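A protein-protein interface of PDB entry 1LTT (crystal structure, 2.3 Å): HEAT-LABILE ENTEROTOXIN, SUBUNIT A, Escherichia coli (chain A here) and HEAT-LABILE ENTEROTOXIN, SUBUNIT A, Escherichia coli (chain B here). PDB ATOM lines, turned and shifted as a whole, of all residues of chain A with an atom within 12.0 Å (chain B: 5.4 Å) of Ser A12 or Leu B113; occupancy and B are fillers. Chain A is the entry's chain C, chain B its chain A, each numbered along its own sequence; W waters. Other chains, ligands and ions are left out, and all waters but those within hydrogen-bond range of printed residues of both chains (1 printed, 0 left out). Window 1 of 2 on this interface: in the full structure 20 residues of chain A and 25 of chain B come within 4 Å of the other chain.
O of Tyr B27 is in hydrogen-bond range of NE2 of Gln A20 (3.0 Å).
OE1 of Gln A9 lies within hydrogen-bond range of N of Ile B36, 3.1 Å away.
The side-chain hydroxyl of Thr A13 is in hydrogen-bond range of the backbone carbonyl oxygen of Gln A9.
O of Ser B111 lies within hydrogen-bond range of N of Phe B92 (2.8 Å).
O of Thr A8 lies within hydrogen-bond range of OG of Ser A12 (2.8 Å).
O of Gly B55 lies within hydrogen-bond range of N of Gly B114.
N of Leu B113 lies within hydrogen-bond range of O of Asn B90 (2.9 Å).
The backbone carbonyl oxygen of Gly B115 lies within hydrogen-bond range of the side-chain amide nitrogen of Asn B90 (3.4 Å).
Among the printed residues, merely in contact across the chains: Tyr A19 with Tyr B27 (3.5 Å), Leu A16 with Leu B113 (3.6 Å), Tyr A15 with Phe B92 (3.6 Å), Ser A12 with Leu B161 (3.6 Å), Tyr A19 with Asn B90 (3.7 Å), Ser A12 with Leu B113 (3.8 Å), Leu A16 with Gly B114 (3.8 Å), Ser A12 with Ile B36 (3.9 Å), Thr A13 with Ile B36 (3.9 Å) and Leu A11 with Leu B161 (3.9 Å).
Cys A4 touches none of the printed residues of chain B.
Glu A7 touches none of the printed residues of chain B.
Printed residues of chain B within 4 Å of Leu A11: Leu B161.
Ser A12 touches three residues of chain B.
Of the printed residues of chain B, Tyr A15 touches Phe B92.
Of the printed residues of chain A, Tyr B27 touches Tyr A19 (3.5 Å) and Gln A20 (3.0 Å).
Of the printed residues of chain A, Ile B36 touches Gln A9, Ser A12 and Thr A13.
No residue of chain A comes within 4 Å of Tyr B56.
Asn B90 touches one residue of chain A.
Phe B92 touches just one residue of chain A: Tyr A15 (3.6 Å).
No residue of chain A comes within 4 Å of Ser B111.
Of the printed residues of chain A, Leu B113 touches Ser A12 and Leu A16.
Gly B114 touches just one residue of chain A: Leu A16.
Of chain A, only Leu A11 (3.9 Å) and Ser A12 (3.6 Å) come within 4 Å of Leu B161.
The nearest residue of chain B that does not touch Ser A12 is Tyr B56 (4.7 Å).
The nearest printed residue of chain B that does not touch Leu A11 is Leu B113 (6.3 Å).
Of the 14 printed residues of chain B, 7 touch a printed residue of chain A.
Hydrophobic or aromatic side chains of chain B within 4 Å of the printed part of chain A: Tyr B27, Ile B36, Phe B92, Leu B113 and Leu B161.
Of the 22 printed residues of chain A, 8 touch a printed residue of chain B.
Printed residues of chain A that touch a printed residue of chain B: Gln A9, Leu A11, Ser A12, Thr A13, Tyr A15, Leu A16, Tyr A19 and Gln A20.
Among the printed residues, 12 pairs touch across the chains.
Water W1 lies within hydrogen-bond range of O of Leu B161, OG of Ser A12 and OH of Tyr B56.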
ATOM      1  N   ASP A   2      -8.642 -34.382   8.087  1.00  0.00           N
ATOM      2  CA  ASP A   2      -9.964 -33.840   8.333  1.00  0.00           C
ATOM      3  C   ASP A   2     -10.965 -34.793   8.947  1.00  0.00           C
ATOM      4  O   ASP A   2     -11.665 -34.266   9.794  1.00  0.00           O
ATOM      5  CB  ASP A   2     -10.600 -33.267   7.044  1.00  0.00           C
ATOM      6  CG  ASP A   2     -11.924 -32.500   7.238  1.00  0.00           C
ATOM      7  OD1 ASP A   2     -12.077 -31.777   8.230  1.00  0.00           O
ATOM      8  OD2 ASP A   2     -12.807 -32.631   6.384  1.00  0.00           O
ATOM      9  N   THR A   3     -11.099 -36.098   8.683  1.00  0.00           N
ATOM     10  CA  THR A   3     -12.207 -36.885   9.228  1.00  0.00           C
ATOM     11  C   THR A   3     -12.498 -36.729  10.708  1.00  0.00           C
ATOM     12  O   THR A   3     -13.671 -36.577  11.020  1.00  0.00           O
ATOM     13  CB  THR A   3     -11.982 -38.374   8.876  1.00  0.00           C
ATOM     14  OG1 THR A   3     -11.848 -38.372   7.449  1.00  0.00           O
ATOM     15  CG2 THR A   3     -13.114 -39.324   9.299  1.00  0.00           C
ATOM     16  N   CYS A   4     -11.519 -36.636  11.600  1.00  0.00           N
ATOM     17  CA  CYS A   4     -11.774 -36.369  13.008  1.00  0.00           C
ATOM     18  C   CYS A   4     -12.560 -35.072  13.155  1.00  0.00           C
ATOM     19  O   CYS A   4     -13.691 -35.008  13.650  1.00  0.00           O
ATOM     20  CB  CYS A   4     -10.454 -36.259  13.712  1.00  0.00           C
ATOM     21  SG  CYS A   4     -10.589 -35.938  15.481  1.00  0.00           S
ATOM     22  N   ASN A   5     -11.981 -34.081  12.489  1.00  0.00           N
ATOM     23  CA  ASN A   5     -12.473 -32.713  12.455  1.00  0.00           C
ATOM     24  C   ASN A   5     -13.843 -32.697  11.806  1.00  0.00           C
ATOM     25  O   ASN A   5     -14.774 -32.110  12.368  1.00  0.00           O
ATOM     26  CB  ASN A   5     -11.581 -31.776  11.622  1.00  0.00           C
ATOM     27  CG  ASN A   5     -10.078 -32.047  11.655  1.00  0.00           C
ATOM     28  OD1 ASN A   5      -9.553 -32.764  12.511  1.00  0.00           O
ATOM     29  ND2 ASN A   5      -9.287 -31.517  10.726  1.00  0.00           N
ATOM     30  N   GLU A   6     -14.024 -33.407  10.682  1.00  0.00           N
ATOM     31  CA  GLU A   6     -15.278 -33.389   9.962  1.00  0.00           C
ATOM     32  C   GLU A   6     -16.318 -34.146  10.762  1.00  0.00           C
ATOM     33  O   GLU A   6     -17.490 -33.770  10.724  1.00  0.00           O
ATOM     34  CB  GLU A   6     -15.126 -34.012   8.565  1.00  0.00           C
ATOM     35  CG  GLU A   6     -15.358 -35.510   8.320  1.00  0.00           C
ATOM     36  CD  GLU A   6     -15.343 -35.928   6.842  1.00  0.00           C
ATOM     37  OE1 GLU A   6     -14.335 -35.702   6.161  1.00  0.00           O
ATOM     38  OE2 GLU A   6     -16.342 -36.490   6.372  1.00  0.00           O
ATOM     39  N   GLU A   7     -15.952 -35.151  11.547  1.00  0.00           N
ATOM     40  CA  GLU A   7     -16.913 -35.852  12.362  1.00  0.00           C
ATOM     41  C   GLU A   7     -17.350 -35.002  13.546  1.00  0.00           C
ATOM     42  O   GLU A   7     -18.540 -35.029  13.874  1.00  0.00           O
ATOM     43  CB  GLU A   7     -16.315 -37.158  12.842  1.00  0.00           C
ATOM     44  CG  GLU A   7     -16.884 -38.326  12.062  1.00  0.00           C
ATOM     45  CD  GLU A   7     -18.281 -38.751  12.531  1.00  0.00           C
ATOM     46  OE1 GLU A   7     -18.380 -39.448  13.550  1.00  0.00           O
ATOM     47  OE2 GLU A   7     -19.267 -38.390  11.873  1.00  0.00           O
ATOM     48  N   THR A   8     -16.474 -34.221  14.201  1.00  0.00           N
ATOM     49  CA  THR A   8     -16.911 -33.354  15.301  1.00  0.00           C
ATOM     50  C   THR A   8     -17.859 -32.283  14.762  1.00  0.00           C
ATOM     51  O   THR A   8     -18.918 -32.039  15.327  1.00  0.00           O
ATOM     52  CB  THR A   8     -15.664 -32.731  15.995  1.00  0.00           C
ATOM     53  OG1 THR A   8     -15.041 -33.791  16.718  1.00  0.00           O
ATOM     54  CG2 THR A   8     -15.999 -31.652  17.018  1.00  0.00           C
ATOM     55  N   GLN A   9     -17.563 -31.708  13.608  1.00  0.00           N
ATOM     56  CA  GLN A   9     -18.463 -30.805  12.950  1.00  0.00           C
ATOM     57  C   GLN A   9     -19.800 -31.504  12.649  1.00  0.00           C
ATOM     58  O   GLN A   9     -20.837 -31.020  13.074  1.00  0.00           O
ATOM     59  CB  GLN A   9     -17.747 -30.353  11.704  1.00  0.00           C
ATOM     60  CG  GLN A   9     -18.484 -29.336  10.857  1.00  0.00           C
ATOM     61  CD  GLN A   9     -18.636 -27.981  11.529  1.00  0.00           C
ATOM     62  OE1 GLN A   9     -17.666 -27.395  12.014  1.00  0.00           O
ATOM     63  NE2 GLN A   9     -19.834 -27.428  11.591  1.00  0.00           N
ATOM     64  N   ASN A  10     -19.861 -32.648  11.964  1.00  0.00           N
ATOM     65  CA  ASN A  10     -21.094 -33.358  11.665  1.00  0.00           C
ATOM     66  C   ASN A  10     -21.869 -33.710  12.925  1.00  0.00           C
ATOM     67  O   ASN A  10     -23.075 -33.479  12.985  1.00  0.00           O
ATOM     68  CB  ASN A  10     -20.761 -34.626  10.871  1.00  0.00           C
ATOM     69  CG  ASN A  10     -21.952 -35.509  10.473  1.00  0.00           C
ATOM     70  OD1 ASN A  10     -22.961 -35.071   9.913  1.00  0.00           O
ATOM     71  ND2 ASN A  10     -21.916 -36.818  10.716  1.00  0.00           N
ATOM     72  N   LEU A  11     -21.235 -34.189  13.994  1.00  0.00           N
ATOM     73  CA  LEU A  11     -21.942 -34.549  15.196  1.00  0.00           C
ATOM     74  C   LEU A  11     -22.486 -33.339  15.933  1.00  0.00           C
ATOM     75  O   LEU A  11     -23.617 -33.375  16.450  1.00  0.00           O
ATOM     76  CB  LEU A  11     -21.039 -35.312  16.131  1.00  0.00           C
ATOM     77  CG  LEU A  11     -20.550 -36.691  15.702  1.00  0.00           C
ATOM     78  CD1 LEU A  11     -19.977 -37.431  16.894  1.00  0.00           C
ATOM     79  CD2 LEU A  11     -21.708 -37.519  15.207  1.00  0.00           C
ATOM     80  N   SER A  12     -21.699 -32.270  16.003  1.00  0.00           N
ATOM     81  CA  SER A  12     -22.119 -31.054  16.653  1.00  0.00           C
ATOM     82  C   SER A  12     -23.246 -30.398  15.866  1.00  0.00           C
ATOM     83  O   SER A  12     -24.170 -29.862  16.483  1.00  0.00           O
ATOM     84  CB  SER A  12     -20.869 -30.175  16.795  1.00  0.00           C
ATOM     85  OG  SER A  12     -19.932 -30.823  17.676  1.00  0.00           O
ATOM     86  N   THR A  13     -23.275 -30.434  14.534  1.00  0.00           N
ATOM     87  CA  THR A  13     -24.413 -29.937  13.759  1.00  0.00           C
ATOM     88  C   THR A  13     -25.663 -30.794  14.005  1.00  0.00           C
ATOM     89  O   THR A  13     -26.745 -30.234  14.163  1.00  0.00           O
ATOM     90  CB  THR A  13     -24.034 -29.913  12.237  1.00  0.00           C
ATOM     91  OG1 THR A  13     -22.904 -29.035  12.087  1.00  0.00           O
ATOM     92  CG2 THR A  13     -25.204 -29.438  11.355  1.00  0.00           C
ATOM     93  N   ILE A  14     -25.584 -32.116  14.111  1.00  0.00           N
ATOM     94  CA  ILE A  14     -26.722 -32.964  14.440  1.00  0.00           C
ATOM     95  C   ILE A  14     -27.365 -32.622  15.783  1.00  0.00           C
ATOM     96  O   ILE A  14     -28.581 -32.441  15.857  1.00  0.00           O
ATOM     97  CB  ILE A  14     -26.265 -34.455  14.428  1.00  0.00           C
ATOM     98  CG1 ILE A  14     -26.087 -34.842  12.966  1.00  0.00           C
ATOM     99  CG2 ILE A  14     -27.234 -35.386  15.157  1.00  0.00           C
ATOM    100  CD1 ILE A  14     -25.321 -36.182  12.910  1.00  0.00           C
ATOM    101  N   TYR A  15     -26.607 -32.559  16.871  1.00  0.00           N
ATOM    102  CA  TYR A  15     -27.156 -32.201  18.187  1.00  0.00           C
ATOM    103  C   TYR A  15     -27.816 -30.797  18.120  1.00  0.00           C
ATOM    104  O   TYR A  15     -28.872 -30.580  18.728  1.00  0.00           O
ATOM    105  CB  TYR A  15     -25.987 -32.260  19.175  1.00  0.00           C
ATOM    106  CG  TYR A  15     -26.272 -32.130  20.660  1.00  0.00           C
ATOM    107  CD1 TYR A  15     -26.647 -30.927  21.237  1.00  0.00           C
ATOM    108  CD2 TYR A  15     -26.175 -33.260  21.425  1.00  0.00           C
ATOM    109  CE1 TYR A  15     -26.924 -30.880  22.580  1.00  0.00           C
ATOM    110  CE2 TYR A  15     -26.450 -33.227  22.765  1.00  0.00           C
ATOM    111  CZ  TYR A  15     -26.822 -32.042  23.319  1.00  0.00           C
ATOM    112  OH  TYR A  15     -27.137 -32.028  24.648  1.00  0.00           O
ATOM    113  N   LEU A  16     -27.250 -29.816  17.395  1.00  0.00           N
ATOM    114  CA  LEU A  16     -27.829 -28.516  17.228  1.00  0.00           C
ATOM    115  C   LEU A  16     -29.082 -28.615  16.407  1.00  0.00           C
ATOM    116  O   LEU A  16     -30.064 -28.098  16.921  1.00  0.00           O
ATOM    117  CB  LEU A  16     -26.894 -27.560  16.516  1.00  0.00           C
ATOM    118  CG  LEU A  16     -27.436 -26.146  16.250  1.00  0.00           C
ATOM    119  CD1 LEU A  16     -27.790 -25.425  17.542  1.00  0.00           C
ATOM    120  CD2 LEU A  16     -26.397 -25.376  15.502  1.00  0.00           C
ATOM    121  N   ARG A  17     -29.154 -29.235  15.216  1.00  0.00           N
ATOM    122  CA  ARG A  17     -30.380 -29.324  14.423  1.00  0.00           C
ATOM    123  C   ARG A  17     -31.497 -29.934  15.261  1.00  0.00           C
ATOM    124  O   ARG A  17     -32.636 -29.452  15.314  1.00  0.00           O
ATOM    125  CB  ARG A  17     -30.159 -30.175  13.225  1.00  0.00           C
ATOM    126  CG  ARG A  17     -29.135 -29.695  12.205  1.00  0.00           C
ATOM    127  CD  ARG A  17     -29.589 -28.449  11.497  1.00  0.00           C
ATOM    128  NE  ARG A  17     -28.551 -27.450  11.630  1.00  0.00           N
ATOM    129  CZ  ARG A  17     -27.841 -26.993  10.591  1.00  0.00           C
ATOM    130  NH1 ARG A  17     -28.063 -27.431   9.341  1.00  0.00           N
ATOM    131  NH2 ARG A  17     -26.872 -26.097  10.826  1.00  0.00           N
ATOM    132  N   GLU A  18     -31.161 -30.919  16.070  1.00  0.00           N
ATOM    133  CA  GLU A  18     -32.111 -31.491  16.993  1.00  0.00           C
ATOM    134  C   GLU A  18     -32.605 -30.540  18.037  1.00  0.00           C
ATOM    135  O   GLU A  18     -33.824 -30.458  18.207  1.00  0.00           O
ATOM    136  CB  GLU A  18     -31.477 -32.676  17.646  1.00  0.00           C
ATOM    137  CG  GLU A  18     -31.617 -33.702  16.540  1.00  0.00           C
ATOM    138  CD  GLU A  18     -31.054 -35.085  16.803  1.00  0.00           C
ATOM    139  OE1 GLU A  18     -30.470 -35.335  17.872  1.00  0.00           O
ATOM    140  OE2 GLU A  18     -31.214 -35.908  15.896  1.00  0.00           O
ATOM    141  N   TYR A  19     -31.753 -29.760  18.725  1.00  0.00           N
ATOM    142  CA  TYR A  19     -32.265 -28.829  19.732  1.00  0.00           C
ATOM    143  C   TYR A  19     -33.120 -27.787  18.999  1.00  0.00           C
ATOM    144  O   TYR A  19     -34.204 -27.424  19.481  1.00  0.00           O
ATOM    145  CB  TYR A  19     -31.094 -28.156  20.499  1.00  0.00           C
ATOM    146  CG  TYR A  19     -31.583 -27.188  21.578  1.00  0.00           C
ATOM    147  CD1 TYR A  19     -32.111 -27.646  22.776  1.00  0.00           C
ATOM    148  CD2 TYR A  19     -31.566 -25.824  21.354  1.00  0.00           C
ATOM    149  CE1 TYR A  19     -32.628 -26.775  23.732  1.00  0.00           C
ATOM    150  CE2 TYR A  19     -32.076 -24.950  22.307  1.00  0.00           C
ATOM    151  CZ  TYR A  19     -32.609 -25.430  23.488  1.00  0.00           C
ATOM    152  OH  TYR A  19     -33.173 -24.575  24.415  1.00  0.00           O
ATOM    153  N   GLN A  20     -32.711 -27.329  17.803  1.00  0.00           N
ATOM    154  CA  GLN A  20     -33.455 -26.331  17.046  1.00  0.00           C
ATOM    155  C   GLN A  20     -34.865 -26.766  16.712  1.00  0.00           C
ATOM    156  O   GLN A  20     -35.750 -25.908  16.720  1.00  0.00           O
ATOM    157  CB  GLN A  20     -32.783 -25.979  15.712  1.00  0.00           C
ATOM    158  CG  GLN A  20     -31.526 -25.193  16.016  1.00  0.00           C
ATOM    159  CD  GLN A  20     -30.883 -24.730  14.738  1.00  0.00           C
ATOM    160  OE1 GLN A  20     -30.563 -25.532  13.877  1.00  0.00           O
ATOM    161  NE2 GLN A  20     -30.654 -23.450  14.541  1.00  0.00           N
ATOM    162  N   SER A  21     -35.063 -28.049  16.381  1.00  0.00           N
ATOM    163  CA  SER A  21     -36.367 -28.623  16.196  1.00  0.00           C
ATOM    164  C   SER A  21     -37.178 -28.509  17.477  1.00  0.00           C
ATOM    165  O   SER A  21     -38.373 -28.207  17.389  1.00  0.00           O
ATOM    166  CB  SER A  21     -36.219 -30.081  15.787  1.00  0.00           C
ATOM    167  OG  SER A  21     -37.535 -30.588  15.591  1.00  0.00           O
ATOM    168  N   LYS A  22     -36.613 -28.710  18.685  1.00  0.00           N
ATOM    169  CA  LYS A  22     -37.377 -28.571  19.923  1.00  0.00           C
ATOM    170  C   LYS A  22     -37.898 -27.172  20.121  1.00  0.00           C
ATOM    171  O   LYS A  22     -39.057 -26.978  20.471  1.00  0.00           O
ATOM    172  CB  LYS A  22     -36.524 -28.938  21.125  1.00  0.00           C
ATOM    173  CG  LYS A  22     -36.264 -30.436  21.137  1.00  0.00           C
ATOM    174  CD  LYS A  22     -37.613 -31.168  20.960  1.00  0.00           C
ATOM    175  CE  LYS A  22     -37.571 -32.698  20.749  1.00  0.00           C
ATOM    176  NZ  LYS A  22     -37.238 -33.442  21.956  1.00  0.00           N
ATOM    177  N   VAL A  23     -37.051 -26.198  19.822  1.00  0.00           N
ATOM    178  CA  VAL A  23     -37.399 -24.770  19.859  1.00  0.00           C
ATOM    179  C   VAL A  23     -38.456 -24.442  18.793  1.00  0.00           C
ATOM    180  O   VAL A  23     -39.433 -23.752  19.103  1.00  0.00           O
ATOM    181  CB  VAL A  23     -36.105 -23.920  19.646  1.00  0.00           C
ATOM    182  CG1 VAL A  23     -36.369 -22.438  19.612  1.00  0.00           C
ATOM    183  CG2 VAL A  23     -35.178 -24.156  20.820  1.00  0.00           C
ATOM    184  N   TYR B  27     -30.535 -17.095  14.371  1.00  0.00           N
ATOM    185  CA  TYR B  27     -30.501 -18.366  15.043  1.00  0.00           C
ATOM    186  C   TYR B  27     -30.810 -19.504  14.094  1.00  0.00           C
ATOM    187  O   TYR B  27     -30.105 -20.509  14.110  1.00  0.00           O
ATOM    188  CB  TYR B  27     -31.508 -18.401  16.179  1.00  0.00           C
ATOM    189  CG  TYR B  27     -31.367 -19.657  17.003  1.00  0.00           C
ATOM    190  CD1 TYR B  27     -30.172 -19.944  17.633  1.00  0.00           C
ATOM    191  CD2 TYR B  27     -32.412 -20.542  17.088  1.00  0.00           C
ATOM    192  CE1 TYR B  27     -30.025 -21.105  18.350  1.00  0.00           C
ATOM    193  CE2 TYR B  27     -32.269 -21.714  17.803  1.00  0.00           C
ATOM    194  CZ  TYR B  27     -31.078 -21.979  18.417  1.00  0.00           C
ATOM    195  OH  TYR B  27     -30.934 -23.136  19.134  1.00  0.00           O
ATOM    196  N   ILE B  36     -18.291 -25.644  14.520  1.00  0.00           N
ATOM    197  CA  ILE B  36     -18.586 -25.832  15.920  1.00  0.00           C
ATOM    198  C   ILE B  36     -17.509 -26.781  16.432  1.00  0.00           C
ATOM    199  O   ILE B  36     -17.272 -27.858  15.866  1.00  0.00           O
ATOM    200  CB  ILE B  36     -20.017 -26.438  16.086  1.00  0.00           C
ATOM    201  CG1 ILE B  36     -21.064 -25.670  15.281  1.00  0.00           C
ATOM    202  CG2 ILE B  36     -20.409 -26.329  17.558  1.00  0.00           C
ATOM    203  CD1 ILE B  36     -22.350 -26.456  14.987  1.00  0.00           C
ATOM    204  N   GLY B  55     -19.043 -21.587  17.081  1.00  0.00           N
ATOM    205  CA  GLY B  55     -20.354 -22.151  17.332  1.00  0.00           C
ATOM    206  C   GLY B  55     -20.842 -22.288  18.772  1.00  0.00           C
ATOM    207  O   GLY B  55     -21.826 -23.003  18.985  1.00  0.00           O
ATOM    208  N   TYR B  56     -20.245 -21.647  19.772  1.00  0.00           N
ATOM    209  CA  TYR B  56     -20.728 -21.701  21.142  1.00  0.00           C
ATOM    210  C   TYR B  56     -20.672 -20.288  21.744  1.00  0.00           C
ATOM    211  O   TYR B  56     -19.801 -19.484  21.379  1.00  0.00           O
ATOM    212  CB  TYR B  56     -19.867 -22.611  22.014  1.00  0.00           C
ATOM    213  CG  TYR B  56     -19.887 -24.132  21.841  1.00  0.00           C
ATOM    214  CD1 TYR B  56     -19.215 -24.764  20.806  1.00  0.00           C
ATOM    215  CD2 TYR B  56     -20.549 -24.889  22.783  1.00  0.00           C
ATOM    216  CE1 TYR B  56     -19.211 -26.142  20.724  1.00  0.00           C
ATOM    217  CE2 TYR B  56     -20.549 -26.271  22.704  1.00  0.00           C
ATOM    218  CZ  TYR B  56     -19.877 -26.889  21.674  1.00  0.00           C
ATOM    219  OH  TYR B  56     -19.857 -28.273  21.616  1.00  0.00           O
ATOM    220  N   VAL B  57     -21.562 -19.959  22.679  1.00  0.00           N
ATOM    221  CA  VAL B  57     -21.592 -18.669  23.354  1.00  0.00           C
ATOM    222  C   VAL B  57     -21.440 -18.966  24.856  1.00  0.00           C
ATOM    223  O   VAL B  57     -22.207 -19.802  25.371  1.00  0.00           O
ATOM    224  CB  VAL B  57     -22.936 -18.000  23.005  1.00  0.00           C
ATOM    225  CG1 VAL B  57     -23.156 -16.786  23.876  1.00  0.00           C
ATOM    226  CG2 VAL B  57     -22.918 -17.505  21.562  1.00  0.00           C
ATOM    227  N   ASN B  90     -28.891 -27.484  25.555  1.00  0.00           N
ATOM    228  CA  ASN B  90     -27.933 -26.985  24.573  1.00  0.00           C
ATOM    229  C   ASN B  90     -26.664 -26.488  25.306  1.00  0.00           C
ATOM    230  O   ASN B  90     -25.660 -26.171  24.682  1.00  0.00           O
ATOM    231  CB  ASN B  90     -28.501 -25.816  23.764  1.00  0.00           C
ATOM    232  CG  ASN B  90     -29.020 -24.590  24.504  1.00  0.00           C
ATOM    233  OD1 ASN B  90     -29.393 -24.641  25.676  1.00  0.00           O
ATOM    234  ND2 ASN B  90     -29.124 -23.445  23.845  1.00  0.00           N
ATOM    235  N   MET B  91     -26.683 -26.417  26.642  1.00  0.00           N
ATOM    236  CA  MET B  91     -25.630 -25.878  27.471  1.00  0.00           C
ATOM    237  C   MET B  91     -24.788 -27.014  28.004  1.00  0.00           C
ATOM    238  O   MET B  91     -25.321 -27.968  28.577  1.00  0.00           O
ATOM    239  CB  MET B  91     -26.145 -25.145  28.711  1.00  0.00           C
ATOM    240  CG  MET B  91     -27.138 -23.988  28.617  1.00  0.00           C
ATOM    241  SD  MET B  91     -26.431 -22.696  27.607  1.00  0.00           S
ATOM    242  CE  MET B  91     -27.388 -21.364  28.259  1.00  0.00           C
ATOM    243  N   PHE B  92     -23.480 -26.773  27.905  1.00  0.00           N
ATOM    244  CA  PHE B  92     -22.420 -27.644  28.360  1.00  0.00           C
ATOM    245  C   PHE B  92     -21.495 -26.936  29.320  1.00  0.00           C
ATOM    246  O   PHE B  92     -20.971 -25.862  29.045  1.00  0.00           O
ATOM    247  CB  PHE B  92     -21.542 -28.140  27.215  1.00  0.00           C
ATOM    248  CG  PHE B  92     -22.302 -29.132  26.368  1.00  0.00           C
ATOM    249  CD1 PHE B  92     -22.359 -30.455  26.767  1.00  0.00           C
ATOM    250  CD2 PHE B  92     -22.964 -28.698  25.234  1.00  0.00           C
ATOM    251  CE1 PHE B  92     -23.092 -31.365  26.030  1.00  0.00           C
ATOM    252  CE2 PHE B  92     -23.688 -29.615  24.512  1.00  0.00           C
ATOM    253  CZ  PHE B  92     -23.753 -30.939  24.906  1.00  0.00           C
ATOM    254  N   SER B 111     -21.173 -23.153  28.120  1.00  0.00           N
ATOM    255  CA  SER B 111     -21.330 -22.726  26.760  1.00  0.00           C
ATOM    256  C   SER B 111     -22.563 -23.336  26.133  1.00  0.00           C
ATOM    257  O   SER B 111     -22.920 -24.475  26.411  1.00  0.00           O
ATOM    258  CB  SER B 111     -20.089 -23.122  25.970  1.00  0.00           C
ATOM    259  OG  SER B 111     -19.006 -22.210  26.127  1.00  0.00           O
ATOM    260  N   ALA B 112     -23.217 -22.557  25.287  1.00  0.00           N
ATOM    261  CA  ALA B 112     -24.414 -22.976  24.583  1.00  0.00           C
ATOM    262  C   ALA B 112     -24.076 -23.340  23.164  1.00  0.00           C
ATOM    263  O   ALA B 112     -23.557 -22.473  22.463  1.00  0.00           O
ATOM    264  CB  ALA B 112     -25.401 -21.848  24.561  1.00  0.00           C
ATOM    265  N   LEU B 113     -24.280 -24.590  22.749  1.00  0.00           N
ATOM    266  CA  LEU B 113     -24.030 -25.072  21.394  1.00  0.00           C
ATOM    267  C   LEU B 113     -25.002 -24.363  20.473  1.00  0.00           C
ATOM    268  O   LEU B 113     -26.216 -24.534  20.613  1.00  0.00           O
ATOM    269  CB  LEU B 113     -24.275 -26.586  21.313  1.00  0.00           C
ATOM    270  CG  LEU B 113     -24.142 -27.598  20.132  1.00  0.00           C
ATOM    271  CD1 LEU B 113     -23.953 -26.917  18.803  1.00  0.00           C
ATOM    272  CD2 LEU B 113     -22.917 -28.463  20.349  1.00  0.00           C
ATOM    273  N   GLY B 114     -24.439 -23.600  19.540  1.00  0.00           N
ATOM    274  CA  GLY B 114     -25.168 -22.881  18.517  1.00  0.00           C
ATOM    275  C   GLY B 114     -25.784 -21.547  18.911  1.00  0.00           C
ATOM    276  O   GLY B 114     -26.489 -20.950  18.077  1.00  0.00           O
ATOM    277  N   GLY B 115     -25.554 -21.006  20.114  1.00  0.00           N
ATOM    278  CA  GLY B 115     -26.194 -19.751  20.470  1.00  0.00           C
ATOM    279  C   GLY B 115     -27.306 -20.003  21.472  1.00  0.00           C
ATOM    280  O   GLY B 115     -27.558 -21.133  21.883  1.00  0.00           O
ATOM    281  N   LEU B 161     -18.388 -34.464  21.645  1.00  0.00           N
ATOM    282  CA  LEU B 161     -18.419 -33.141  21.046  1.00  0.00           C
ATOM    283  C   LEU B 161     -17.237 -32.289  21.524  1.00  0.00           C
ATOM    284  O   LEU B 161     -17.129 -31.128  21.117  1.00  0.00           O
ATOM    285  CB  LEU B 161     -19.732 -32.440  21.407  1.00  0.00           C
ATOM    286  CG  LEU B 161     -20.999 -33.193  21.134  1.00  0.00           C
ATOM    287  CD1 LEU B 161     -22.199 -32.313  21.438  1.00  0.00           C
ATOM    288  CD2 LEU B 161     -21.001 -33.649  19.695  1.00  0.00           C
HETATM  289  O   HOH W   1     -18.196 -29.240  19.285  1.00  0.00           O
